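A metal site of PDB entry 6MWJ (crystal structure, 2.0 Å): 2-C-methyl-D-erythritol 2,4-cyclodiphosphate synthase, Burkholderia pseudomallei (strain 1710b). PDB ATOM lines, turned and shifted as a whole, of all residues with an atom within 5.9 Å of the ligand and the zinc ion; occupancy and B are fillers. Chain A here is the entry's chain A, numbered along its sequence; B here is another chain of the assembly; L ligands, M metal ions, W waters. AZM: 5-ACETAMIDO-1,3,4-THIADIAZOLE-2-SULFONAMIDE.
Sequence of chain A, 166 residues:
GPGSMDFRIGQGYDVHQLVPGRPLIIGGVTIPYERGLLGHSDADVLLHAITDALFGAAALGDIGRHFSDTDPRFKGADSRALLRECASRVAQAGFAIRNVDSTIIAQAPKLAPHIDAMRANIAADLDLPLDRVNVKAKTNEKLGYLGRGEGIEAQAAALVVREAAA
Water W3 bridges N of Gly 64 (3.1 Å) and N3 of the ligand (3.1 Å).
Water W2 lies within hydrogen-bond range of the backbone NH of Thr 139 of chain B (3.1 Å) and a nitrogen (N1) of the ligand (3.2 Å).
Water W1 lies within hydrogen-bond range of OG of Ser 41, OD1 of Asp 69, N of His 40 and O3 of the ligand.
The zinc ion is bound by a ring nitrogen (NE2) of His 16 (1.9 Å), the side-chain carboxylate of Asp 14 (2.0 Å), an oxygen (O1) of the ligand (2.0 Å) and a ring nitrogen (ND1) of His 48 (2.1 Å).
An oxygen (O3) of the ligand is in hydrogen-bond range of the side-chain hydroxyl (OG) of Ser 41 (3.3 Å).
The side-chain amino group (NZ) of Lys 138 of chain B lies within hydrogen-bond range of an oxygen (O2) of the ligand.
O of Phe 67 lies within hydrogen-bond range of N4 of the ligand, at 2.7 Å.
The side-chain carboxylate (OD1) of Asp 69 lies within hydrogen-bond range of a nitrogen (N4) of the ligand, at 3.2 Å.
Within 4 Å of the zinc ion: Asp 14, His 16 and His 48.
Ile 63 touches the ligand (CG2 to O2, 3.3 Å).
Gly 64 touches the ligand.
Ser 68 touches the ligand.
CB of Phe 74 touches C4 of the ligand (3.6 Å).
CD1 of Leu 82 touches O3 of the ligand, 3.6 Å away.
Hydrophobic or aromatic side chains within 4 Å of the ligand: His 16, His 48, Ile 63, Phe 67, Phe 74 and Leu 82.
Within 4 Å of the ligand: Asp 14, His 16, Ser 41, His 48, Ile 63, Gly 64, Phe 67, Ser 68, Asp 69, Phe 74, Leu 82 and Lys 138 of chain B.
The side-chain amino group of Lys 138 of chain B lies within salt-bridge range of the side-chain carboxylate of Asp 52, 3.3 Å away.
NE2 of His 48 lies within hydrogen-bond range of OG of Ser 79.
A ring nitrogen (NE2) of His 48 lies close to the side-chain hydroxyl of Ser 41, at 3.3 Å.
The side-chain amino group of Lys 138 of chain B lies within hydrogen-bond range of the backbone carbonyl oxygen of Tyr 13 (2.7 Å).
OG of Ser 41 sits close to N of Ala 43, at 3.0 Å.
N of Ile 63 lies within hydrogen-bond range of OD1 of Asp 52 (2.9 Å).
The side-chain carboxylate (OD1) of Asp 14 lies within salt-bridge range of the side-chain amino group (NZ) of Lys 138 of chain B.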
ATOM      1  N   TYR A  13      -3.180 -36.469 -28.477  1.00  0.00           N
ATOM      2  CA  TYR A  13      -2.507 -37.172 -27.385  1.00  0.00           C
ATOM      3  C   TYR A  13      -2.581 -36.296 -26.146  1.00  0.00           C
ATOM      4  O   TYR A  13      -2.484 -35.067 -26.245  1.00  0.00           O
ATOM      5  CB  TYR A  13      -1.027 -37.478 -27.727  1.00  0.00           C
ATOM      6  CG  TYR A  13      -0.183 -37.928 -26.551  1.00  0.00           C
ATOM      7  CD1 TYR A  13      -0.104 -39.280 -26.206  1.00  0.00           C
ATOM      8  CD2 TYR A  13       0.554 -37.009 -25.790  1.00  0.00           C
ATOM      9  CE1 TYR A  13       0.662 -39.704 -25.132  1.00  0.00           C
ATOM     10  CE2 TYR A  13       1.314 -37.429 -24.701  1.00  0.00           C
ATOM     11  CZ  TYR A  13       1.378 -38.783 -24.395  1.00  0.00           C
ATOM     12  OH  TYR A  13       2.134 -39.215 -23.324  1.00  0.00           O
ATOM     13  N   ASP A  14      -2.761 -36.911 -24.978  1.00  0.00           N
ATOM     14  CA  ASP A  14      -2.627 -36.143 -23.743  1.00  0.00           C
ATOM     15  C   ASP A  14      -2.288 -37.087 -22.593  1.00  0.00           C
ATOM     16  O   ASP A  14      -2.593 -38.277 -22.641  1.00  0.00           O
ATOM     17  CB  ASP A  14      -3.902 -35.344 -23.431  1.00  0.00           C
ATOM     18  CG  ASP A  14      -3.637 -34.169 -22.506  1.00  0.00           C
ATOM     19  OD1 ASP A  14      -2.502 -33.647 -22.522  1.00  0.00           O
ATOM     20  OD2 ASP A  14      -4.533 -33.788 -21.747  1.00  0.00           O
ATOM     21  N   VAL A  15      -1.660 -36.526 -21.558  1.00  0.00           N
ATOM     22  CA  VAL A  15      -1.366 -37.232 -20.308  1.00  0.00           C
ATOM     23  C   VAL A  15      -1.427 -36.221 -19.170  1.00  0.00           C
ATOM     24  O   VAL A  15      -1.074 -35.052 -19.337  1.00  0.00           O
ATOM     25  CB  VAL A  15       0.009 -37.945 -20.367  1.00  0.00           C
ATOM     26  CG1 VAL A  15       1.158 -36.948 -20.353  1.00  0.00           C
ATOM     27  CG2 VAL A  15       0.140 -38.931 -19.224  1.00  0.00           C
ATOM     28  N   HIS A  16      -1.891 -36.671 -18.002  1.00  0.00           N
ATOM     29  CA  HIS A  16      -1.829 -35.850 -16.796  1.00  0.00           C
ATOM     30  C   HIS A  16      -1.451 -36.741 -15.635  1.00  0.00           C
ATOM     31  O   HIS A  16      -1.822 -37.922 -15.597  1.00  0.00           O
ATOM     32  CB  HIS A  16      -3.169 -35.165 -16.476  1.00  0.00           C
ATOM     33  CG  HIS A  16      -3.482 -34.022 -17.392  1.00  0.00           C
ATOM     34  ND1 HIS A  16      -3.177 -32.712 -17.075  1.00  0.00           N
ATOM     35  CD2 HIS A  16      -4.078 -33.997 -18.615  1.00  0.00           C
ATOM     36  CE1 HIS A  16      -3.575 -31.923 -18.068  1.00  0.00           C
ATOM     37  NE2 HIS A  16      -4.123 -32.674 -19.008  1.00  0.00           N
ATOM     38  N   HIS A  40      -3.978 -27.312 -14.969  1.00  0.00           N
ATOM     39  CA  HIS A  40      -4.501 -25.950 -14.796  1.00  0.00           C
ATOM     40  C   HIS A  40      -6.020 -25.931 -14.921  1.00  0.00           C
ATOM     41  O   HIS A  40      -6.719 -25.340 -14.094  1.00  0.00           O
ATOM     42  CB  HIS A  40      -3.853 -25.022 -15.823  1.00  0.00           C
ATOM     43  CG  HIS A  40      -4.215 -23.576 -15.650  1.00  0.00           C
ATOM     44  ND1 HIS A  40      -3.776 -22.820 -14.585  1.00  0.00           N
ATOM     45  CD2 HIS A  40      -4.962 -22.754 -16.427  1.00  0.00           C
ATOM     46  CE1 HIS A  40      -4.244 -21.581 -14.714  1.00  0.00           C
ATOM     47  NE2 HIS A  40      -4.960 -21.521 -15.812  1.00  0.00           N
ATOM     48  N   SER A  41      -6.555 -26.602 -15.949  1.00  0.00           N
ATOM     49  CA  SER A  41      -7.992 -26.799 -16.082  1.00  0.00           C
ATOM     50  C   SER A  41      -8.446 -27.916 -15.150  1.00  0.00           C
ATOM     51  O   SER A  41      -7.720 -28.279 -14.210  1.00  0.00           O
ATOM     52  CB  SER A  41      -8.371 -27.148 -17.522  1.00  0.00           C
ATOM     53  OG  SER A  41      -7.819 -28.418 -17.903  1.00  0.00           O
ATOM     54  N   ALA A  43      -8.243 -30.767 -16.052  1.00  0.00           N
ATOM     55  CA  ALA A  43      -7.269 -31.794 -16.425  1.00  0.00           C
ATOM     56  C   ALA A  43      -7.922 -33.017 -17.079  1.00  0.00           C
ATOM     57  O   ALA A  43      -7.363 -34.125 -17.001  1.00  0.00           O
ATOM     58  CB  ALA A  43      -6.415 -32.245 -15.218  1.00  0.00           C
ATOM     59  N   ASP A  44      -9.059 -32.836 -17.736  1.00  0.00           N
ATOM     60  CA  ASP A  44      -9.750 -33.927 -18.423  1.00  0.00           C
ATOM     61  C   ASP A  44      -8.929 -34.428 -19.598  1.00  0.00           C
ATOM     62  O   ASP A  44      -9.037 -33.889 -20.716  1.00  0.00           O
ATOM     63  CB  ASP A  44     -11.139 -33.461 -18.868  1.00  0.00           C
ATOM     64  CG  ASP A  44     -12.053 -34.608 -19.251  1.00  0.00           C
ATOM     65  OD1 ASP A  44     -11.566 -35.569 -19.882  1.00  0.00           O
ATOM     66  OD2 ASP A  44     -13.268 -34.541 -18.938  1.00  0.00           O
ATOM     67  N   VAL A  45      -8.133 -35.475 -19.380  1.00  0.00           N
ATOM     68  CA  VAL A  45      -7.137 -35.909 -20.366  1.00  0.00           C
ATOM     69  C   VAL A  45      -7.802 -36.422 -21.640  1.00  0.00           C
ATOM     70  O   VAL A  45      -7.278 -36.221 -22.748  1.00  0.00           O
ATOM     71  CB  VAL A  45      -6.204 -36.967 -19.726  1.00  0.00           C
ATOM     72  CG1 VAL A  45      -6.985 -38.228 -19.349  1.00  0.00           C
ATOM     73  CG2 VAL A  45      -5.039 -37.300 -20.648  1.00  0.00           C
ATOM     74  N   HIS A  48      -9.124 -33.332 -23.691  1.00  0.00           N
ATOM     75  CA  HIS A  48      -7.994 -32.595 -24.258  1.00  0.00           C
ATOM     76  C   HIS A  48      -7.451 -33.295 -25.490  1.00  0.00           C
ATOM     77  O   HIS A  48      -7.146 -32.642 -26.504  1.00  0.00           O
ATOM     78  CB  HIS A  48      -6.885 -32.434 -23.213  1.00  0.00           C
ATOM     79  CG  HIS A  48      -7.260 -31.552 -22.057  1.00  0.00           C
ATOM     80  ND1 HIS A  48      -6.368 -31.243 -21.048  1.00  0.00           N
ATOM     81  CD2 HIS A  48      -8.412 -30.912 -21.756  1.00  0.00           C
ATOM     82  CE1 HIS A  48      -6.961 -30.453 -20.179  1.00  0.00           C
ATOM     83  NE2 HIS A  48      -8.202 -30.240 -20.579  1.00  0.00           N
ATOM     84  N   ALA A  49      -7.318 -34.620 -25.435  1.00  0.00           N
ATOM     85  CA  ALA A  49      -6.868 -35.380 -26.595  1.00  0.00           C
ATOM     86  C   ALA A  49      -7.834 -35.226 -27.769  1.00  0.00           C
ATOM     87  O   ALA A  49      -7.412 -35.017 -28.912  1.00  0.00           O
ATOM     88  CB  ALA A  49      -6.705 -36.851 -26.225  1.00  0.00           C
ATOM     89  N   ASP A  52      -7.555 -31.715 -29.257  1.00  0.00           N
ATOM     90  CA  ASP A  52      -6.380 -31.607 -30.113  1.00  0.00           C
ATOM     91  C   ASP A  52      -6.621 -32.252 -31.470  1.00  0.00           C
ATOM     92  O   ASP A  52      -6.209 -31.707 -32.498  1.00  0.00           O
ATOM     93  CB  ASP A  52      -5.155 -32.261 -29.440  1.00  0.00           C
ATOM     94  CG  ASP A  52      -4.099 -31.254 -29.025  1.00  0.00           C
ATOM     95  OD1 ASP A  52      -4.353 -30.032 -29.148  1.00  0.00           O
ATOM     96  OD2 ASP A  52      -3.007 -31.682 -28.565  1.00  0.00           O
ATOM     97  N   ILE A  63      -4.707 -27.185 -28.643  1.00  0.00           N
ATOM     98  CA  ILE A  63      -5.539 -26.716 -27.538  1.00  0.00           C
ATOM     99  C   ILE A  63      -4.843 -25.599 -26.777  1.00  0.00           C
ATOM    100  O   ILE A  63      -5.487 -24.640 -26.336  1.00  0.00           O
ATOM    101  CB  ILE A  63      -5.892 -27.906 -26.625  1.00  0.00           C
ATOM    102  CG1 ILE A  63      -6.809 -27.457 -25.488  1.00  0.00           C
ATOM    103  CG2 ILE A  63      -4.612 -28.633 -26.122  1.00  0.00           C
ATOM    104  CD1 ILE A  63      -7.354 -28.614 -24.634  1.00  0.00           C
ATOM    105  N   GLY A  64      -3.516 -25.663 -26.645  1.00  0.00           N
ATOM    106  CA  GLY A  64      -2.778 -24.611 -25.965  1.00  0.00           C
ATOM    107  C   GLY A  64      -2.788 -23.289 -26.702  1.00  0.00           C
ATOM    108  O   GLY A  64      -2.804 -22.223 -26.083  1.00  0.00           O
ATOM    109  N   ARG A  65      -2.771 -23.334 -28.039  1.00  0.00           N
ATOM    110  CA  ARG A  65      -2.946 -22.115 -28.819  1.00  0.00           C
ATOM    111  C   ARG A  65      -4.304 -21.472 -28.550  1.00  0.00           C
ATOM    112  O   ARG A  65      -4.410 -20.251 -28.439  1.00  0.00           O
ATOM    113  CB  ARG A  65      -2.805 -22.415 -30.312  1.00  0.00           C
ATOM    114  CG  ARG A  65      -3.293 -21.284 -31.202  1.00  0.00           C
ATOM    115  CD  ARG A  65      -3.074 -21.570 -32.662  1.00  0.00           C
ATOM    116  NE  ARG A  65      -4.088 -20.939 -33.494  1.00  0.00           N
ATOM    117  CZ  ARG A  65      -4.124 -21.026 -34.825  1.00  0.00           C
ATOM    118  NH1 ARG A  65      -5.093 -20.408 -35.501  1.00  0.00           N
ATOM    119  NH2 ARG A  65      -3.185 -21.729 -35.471  1.00  0.00           N
ATOM    120  N   PHE A  67      -6.612 -22.152 -25.946  1.00  0.00           N
ATOM    121  CA  PHE A  67      -6.966 -21.944 -24.540  1.00  0.00           C
ATOM    122  C   PHE A  67      -5.675 -22.032 -23.711  1.00  0.00           C
ATOM    123  O   PHE A  67      -5.244 -23.132 -23.355  1.00  0.00           O
ATOM    124  CB  PHE A  67      -7.992 -22.985 -24.093  1.00  0.00           C
ATOM    125  CG  PHE A  67      -9.099 -23.243 -25.092  1.00  0.00           C
ATOM    126  CD1 PHE A  67     -10.076 -22.275 -25.347  1.00  0.00           C
ATOM    127  CD2 PHE A  67      -9.195 -24.462 -25.749  1.00  0.00           C
ATOM    128  CE1 PHE A  67     -11.106 -22.522 -26.240  1.00  0.00           C
ATOM    129  CE2 PHE A  67     -10.224 -24.709 -26.642  1.00  0.00           C
ATOM    130  CZ  PHE A  67     -11.179 -23.739 -26.888  1.00  0.00           C
ATOM    131  N   SER A  68      -5.087 -20.878 -23.384  1.00  0.00           N
ATOM    132  CA  SER A  68      -3.815 -20.828 -22.672  1.00  0.00           C
ATOM    133  C   SER A  68      -3.850 -21.617 -21.370  1.00  0.00           C
ATOM    134  O   SER A  68      -4.750 -21.432 -20.549  1.00  0.00           O
ATOM    135  CB  SER A  68      -3.445 -19.373 -22.383  1.00  0.00           C
ATOM    136  OG  SER A  68      -2.373 -19.282 -21.441  1.00  0.00           O
ATOM    137  N   ASP A  69      -2.856 -22.483 -21.173  1.00  0.00           N
ATOM    138  CA  ASP A  69      -2.805 -23.324 -19.982  1.00  0.00           C
ATOM    139  C   ASP A  69      -2.216 -22.614 -18.769  1.00  0.00           C
ATOM    140  O   ASP A  69      -2.008 -23.249 -17.735  1.00  0.00           O
ATOM    141  CB  ASP A  69      -2.007 -24.608 -20.256  1.00  0.00           C
ATOM    142  CG  ASP A  69      -2.598 -25.821 -19.540  1.00  0.00           C
ATOM    143  OD1 ASP A  69      -3.813 -25.805 -19.227  1.00  0.00           O
ATOM    144  OD2 ASP A  69      -1.852 -26.800 -19.285  1.00  0.00           O
ATOM    145  N   PHE A  74      -8.764 -19.711 -17.001  1.00  0.00           N
ATOM    146  CA  PHE A  74      -8.984 -21.130 -17.283  1.00  0.00           C
ATOM    147  C   PHE A  74      -8.625 -22.015 -16.100  1.00  0.00           C
ATOM    148  O   PHE A  74      -8.604 -23.242 -16.241  1.00  0.00           O
ATOM    149  CB  PHE A  74      -8.187 -21.559 -18.520  1.00  0.00           C
ATOM    150  CG  PHE A  74      -8.686 -20.962 -19.811  1.00  0.00           C
ATOM    151  CD1 PHE A  74     -10.019 -21.102 -20.199  1.00  0.00           C
ATOM    152  CD2 PHE A  74      -7.828 -20.259 -20.646  1.00  0.00           C
ATOM    153  CE1 PHE A  74     -10.469 -20.553 -21.388  1.00  0.00           C
ATOM    154  CE2 PHE A  74      -8.271 -19.704 -21.841  1.00  0.00           C
ATOM    155  CZ  PHE A  74      -9.601 -19.869 -22.214  1.00  0.00           C
ATOM    156  N   ALA A  77     -10.973 -24.753 -15.390  1.00  0.00           N
ATOM    157  CA  ALA A  77     -11.914 -24.694 -16.508  1.00  0.00           C
ATOM    158  C   ALA A  77     -12.553 -26.051 -16.778  1.00  0.00           C
ATOM    159  O   ALA A  77     -11.914 -27.100 -16.692  1.00  0.00           O
ATOM    160  CB  ALA A  77     -11.217 -24.190 -17.759  1.00  0.00           C
ATOM    161  N   SER A  79     -13.519 -28.731 -19.058  1.00  0.00           N
ATOM    162  CA  SER A  79     -12.993 -29.109 -20.370  1.00  0.00           C
ATOM    163  C   SER A  79     -14.076 -29.463 -21.371  1.00  0.00           C
ATOM    164  O   SER A  79     -13.776 -29.565 -22.567  1.00  0.00           O
ATOM    165  CB  SER A  79     -11.986 -30.256 -20.243  1.00  0.00           C
ATOM    166  OG  SER A  79     -10.765 -29.816 -19.633  1.00  0.00           O
ATOM    167  N   LEU A  82     -14.525 -26.191 -23.076  1.00  0.00           N
ATOM    168  CA  LEU A  82     -13.440 -26.014 -24.039  1.00  0.00           C
ATOM    169  C   LEU A  82     -13.683 -26.850 -25.287  1.00  0.00           C
ATOM    170  O   LEU A  82     -13.472 -26.371 -26.417  1.00  0.00           O
ATOM    171  CB  LEU A  82     -12.091 -26.373 -23.405  1.00  0.00           C
ATOM    172  CG  LEU A  82     -11.640 -25.612 -22.146  1.00  0.00           C
ATOM    173  CD1 LEU A  82     -10.248 -26.108 -21.672  1.00  0.00           C
ATOM    174  CD2 LEU A  82     -11.618 -24.104 -22.387  1.00  0.00           C
ATOM    175  N   LYS B 138       3.294 -30.203 -27.093  1.00  0.00           N
ATOM    176  CA  LYS B 138       2.917 -30.191 -25.685  1.00  0.00           C
ATOM    177  C   LYS B 138       3.963 -30.945 -24.878  1.00  0.00           C
ATOM    178  O   LYS B 138       4.761 -31.710 -25.436  1.00  0.00           O
ATOM    179  CB  LYS B 138       1.545 -30.819 -25.477  1.00  0.00           C
ATOM    180  CG  LYS B 138       1.509 -32.289 -25.882  1.00  0.00           C
ATOM    181  CD  LYS B 138       0.177 -32.931 -25.526  1.00  0.00           C
ATOM    182  CE  LYS B 138      -0.970 -32.138 -26.102  1.00  0.00           C
ATOM    183  NZ  LYS B 138      -2.279 -32.450 -25.484  1.00  0.00           N
ATOM    184  N   THR B 139       3.953 -30.737 -23.562  1.00  0.00           N
ATOM    185  CA  THR B 139       4.865 -31.455 -22.682  1.00  0.00           C
ATOM    186  C   THR B 139       4.276 -32.820 -22.325  1.00  0.00           C
ATOM    187  O   THR B 139       3.143 -33.159 -22.678  1.00  0.00           O
ATOM    188  CB  THR B 139       5.135 -30.657 -21.406  1.00  0.00           C
ATOM    189  OG1 THR B 139       3.994 -30.740 -20.540  1.00  0.00           O
ATOM    190  CG2 THR B 139       5.400 -29.179 -21.715  1.00  0.00           C
ATOM    191  N   GLU B 141       4.033 -33.612 -19.068  1.00  0.00           N
ATOM    192  CA  GLU B 141       3.662 -33.417 -17.661  1.00  0.00           C
ATOM    193  C   GLU B 141       4.672 -34.062 -16.716  1.00  0.00           C
ATOM    194  O   GLU B 141       4.317 -34.605 -15.674  1.00  0.00           O
ATOM    195  CB  GLU B 141       2.248 -33.939 -17.381  1.00  0.00           C
ATOM    196  CG  GLU B 141       1.180 -33.190 -18.126  1.00  0.00           C
ATOM    197  CD  GLU B 141       1.110 -31.756 -17.695  1.00  0.00           C
ATOM    198  OE1 GLU B 141       1.079 -31.492 -16.476  1.00  0.00           O
ATOM    199  OE2 GLU B 141       1.103 -30.883 -18.587  1.00  0.00           O
HETATM  200  C1  AZM L   1      -3.516 -28.443 -22.639  1.00  0.00           C
HETATM  201  C2  AZM L   1      -4.671 -26.388 -22.291  1.00  0.00           C
HETATM  202  C3  AZM L   1      -6.567 -25.514 -20.964  1.00  0.00           C
HETATM  203  C4  AZM L   1      -7.246 -24.179 -20.739  1.00  0.00           C
HETATM  204  N1  AZM L   1      -1.328 -29.985 -22.963  1.00  0.00           N
HETATM  205  N2  AZM L   1      -3.649 -26.249 -23.063  1.00  0.00           N
HETATM  206  N3  AZM L   1      -2.984 -27.497 -23.266  1.00  0.00           N
HETATM  207  N4  AZM L   1      -5.498 -25.397 -21.879  1.00  0.00           N
HETATM  208  O1  AZM L   1      -3.148 -30.639 -21.187  1.00  0.00           O
HETATM  209  O2  AZM L   1      -3.719 -30.902 -23.835  1.00  0.00           O
HETATM  210  O3  AZM L   1      -6.882 -26.540 -20.437  1.00  0.00           O
HETATM  211  S1  AZM L   1      -2.980 -30.143 -22.677  1.00  0.00           S
HETATM  212  S2  AZM L   1      -4.968 -28.071 -21.673  1.00  0.00           S
HETATM  213 ZN    ZN M   1      -4.471 -32.064 -20.776  1.00  0.00          ZN
HETATM  214  O   HOH W   1      -5.033 -28.211 -18.027  1.00  0.00           O
HETATM  215  O   HOH W   2       1.646 -28.753 -22.749  1.00  0.00           O
HETATM  216  O   HOH W   3      -1.265 -27.572 -25.865  1.00  0.00           O
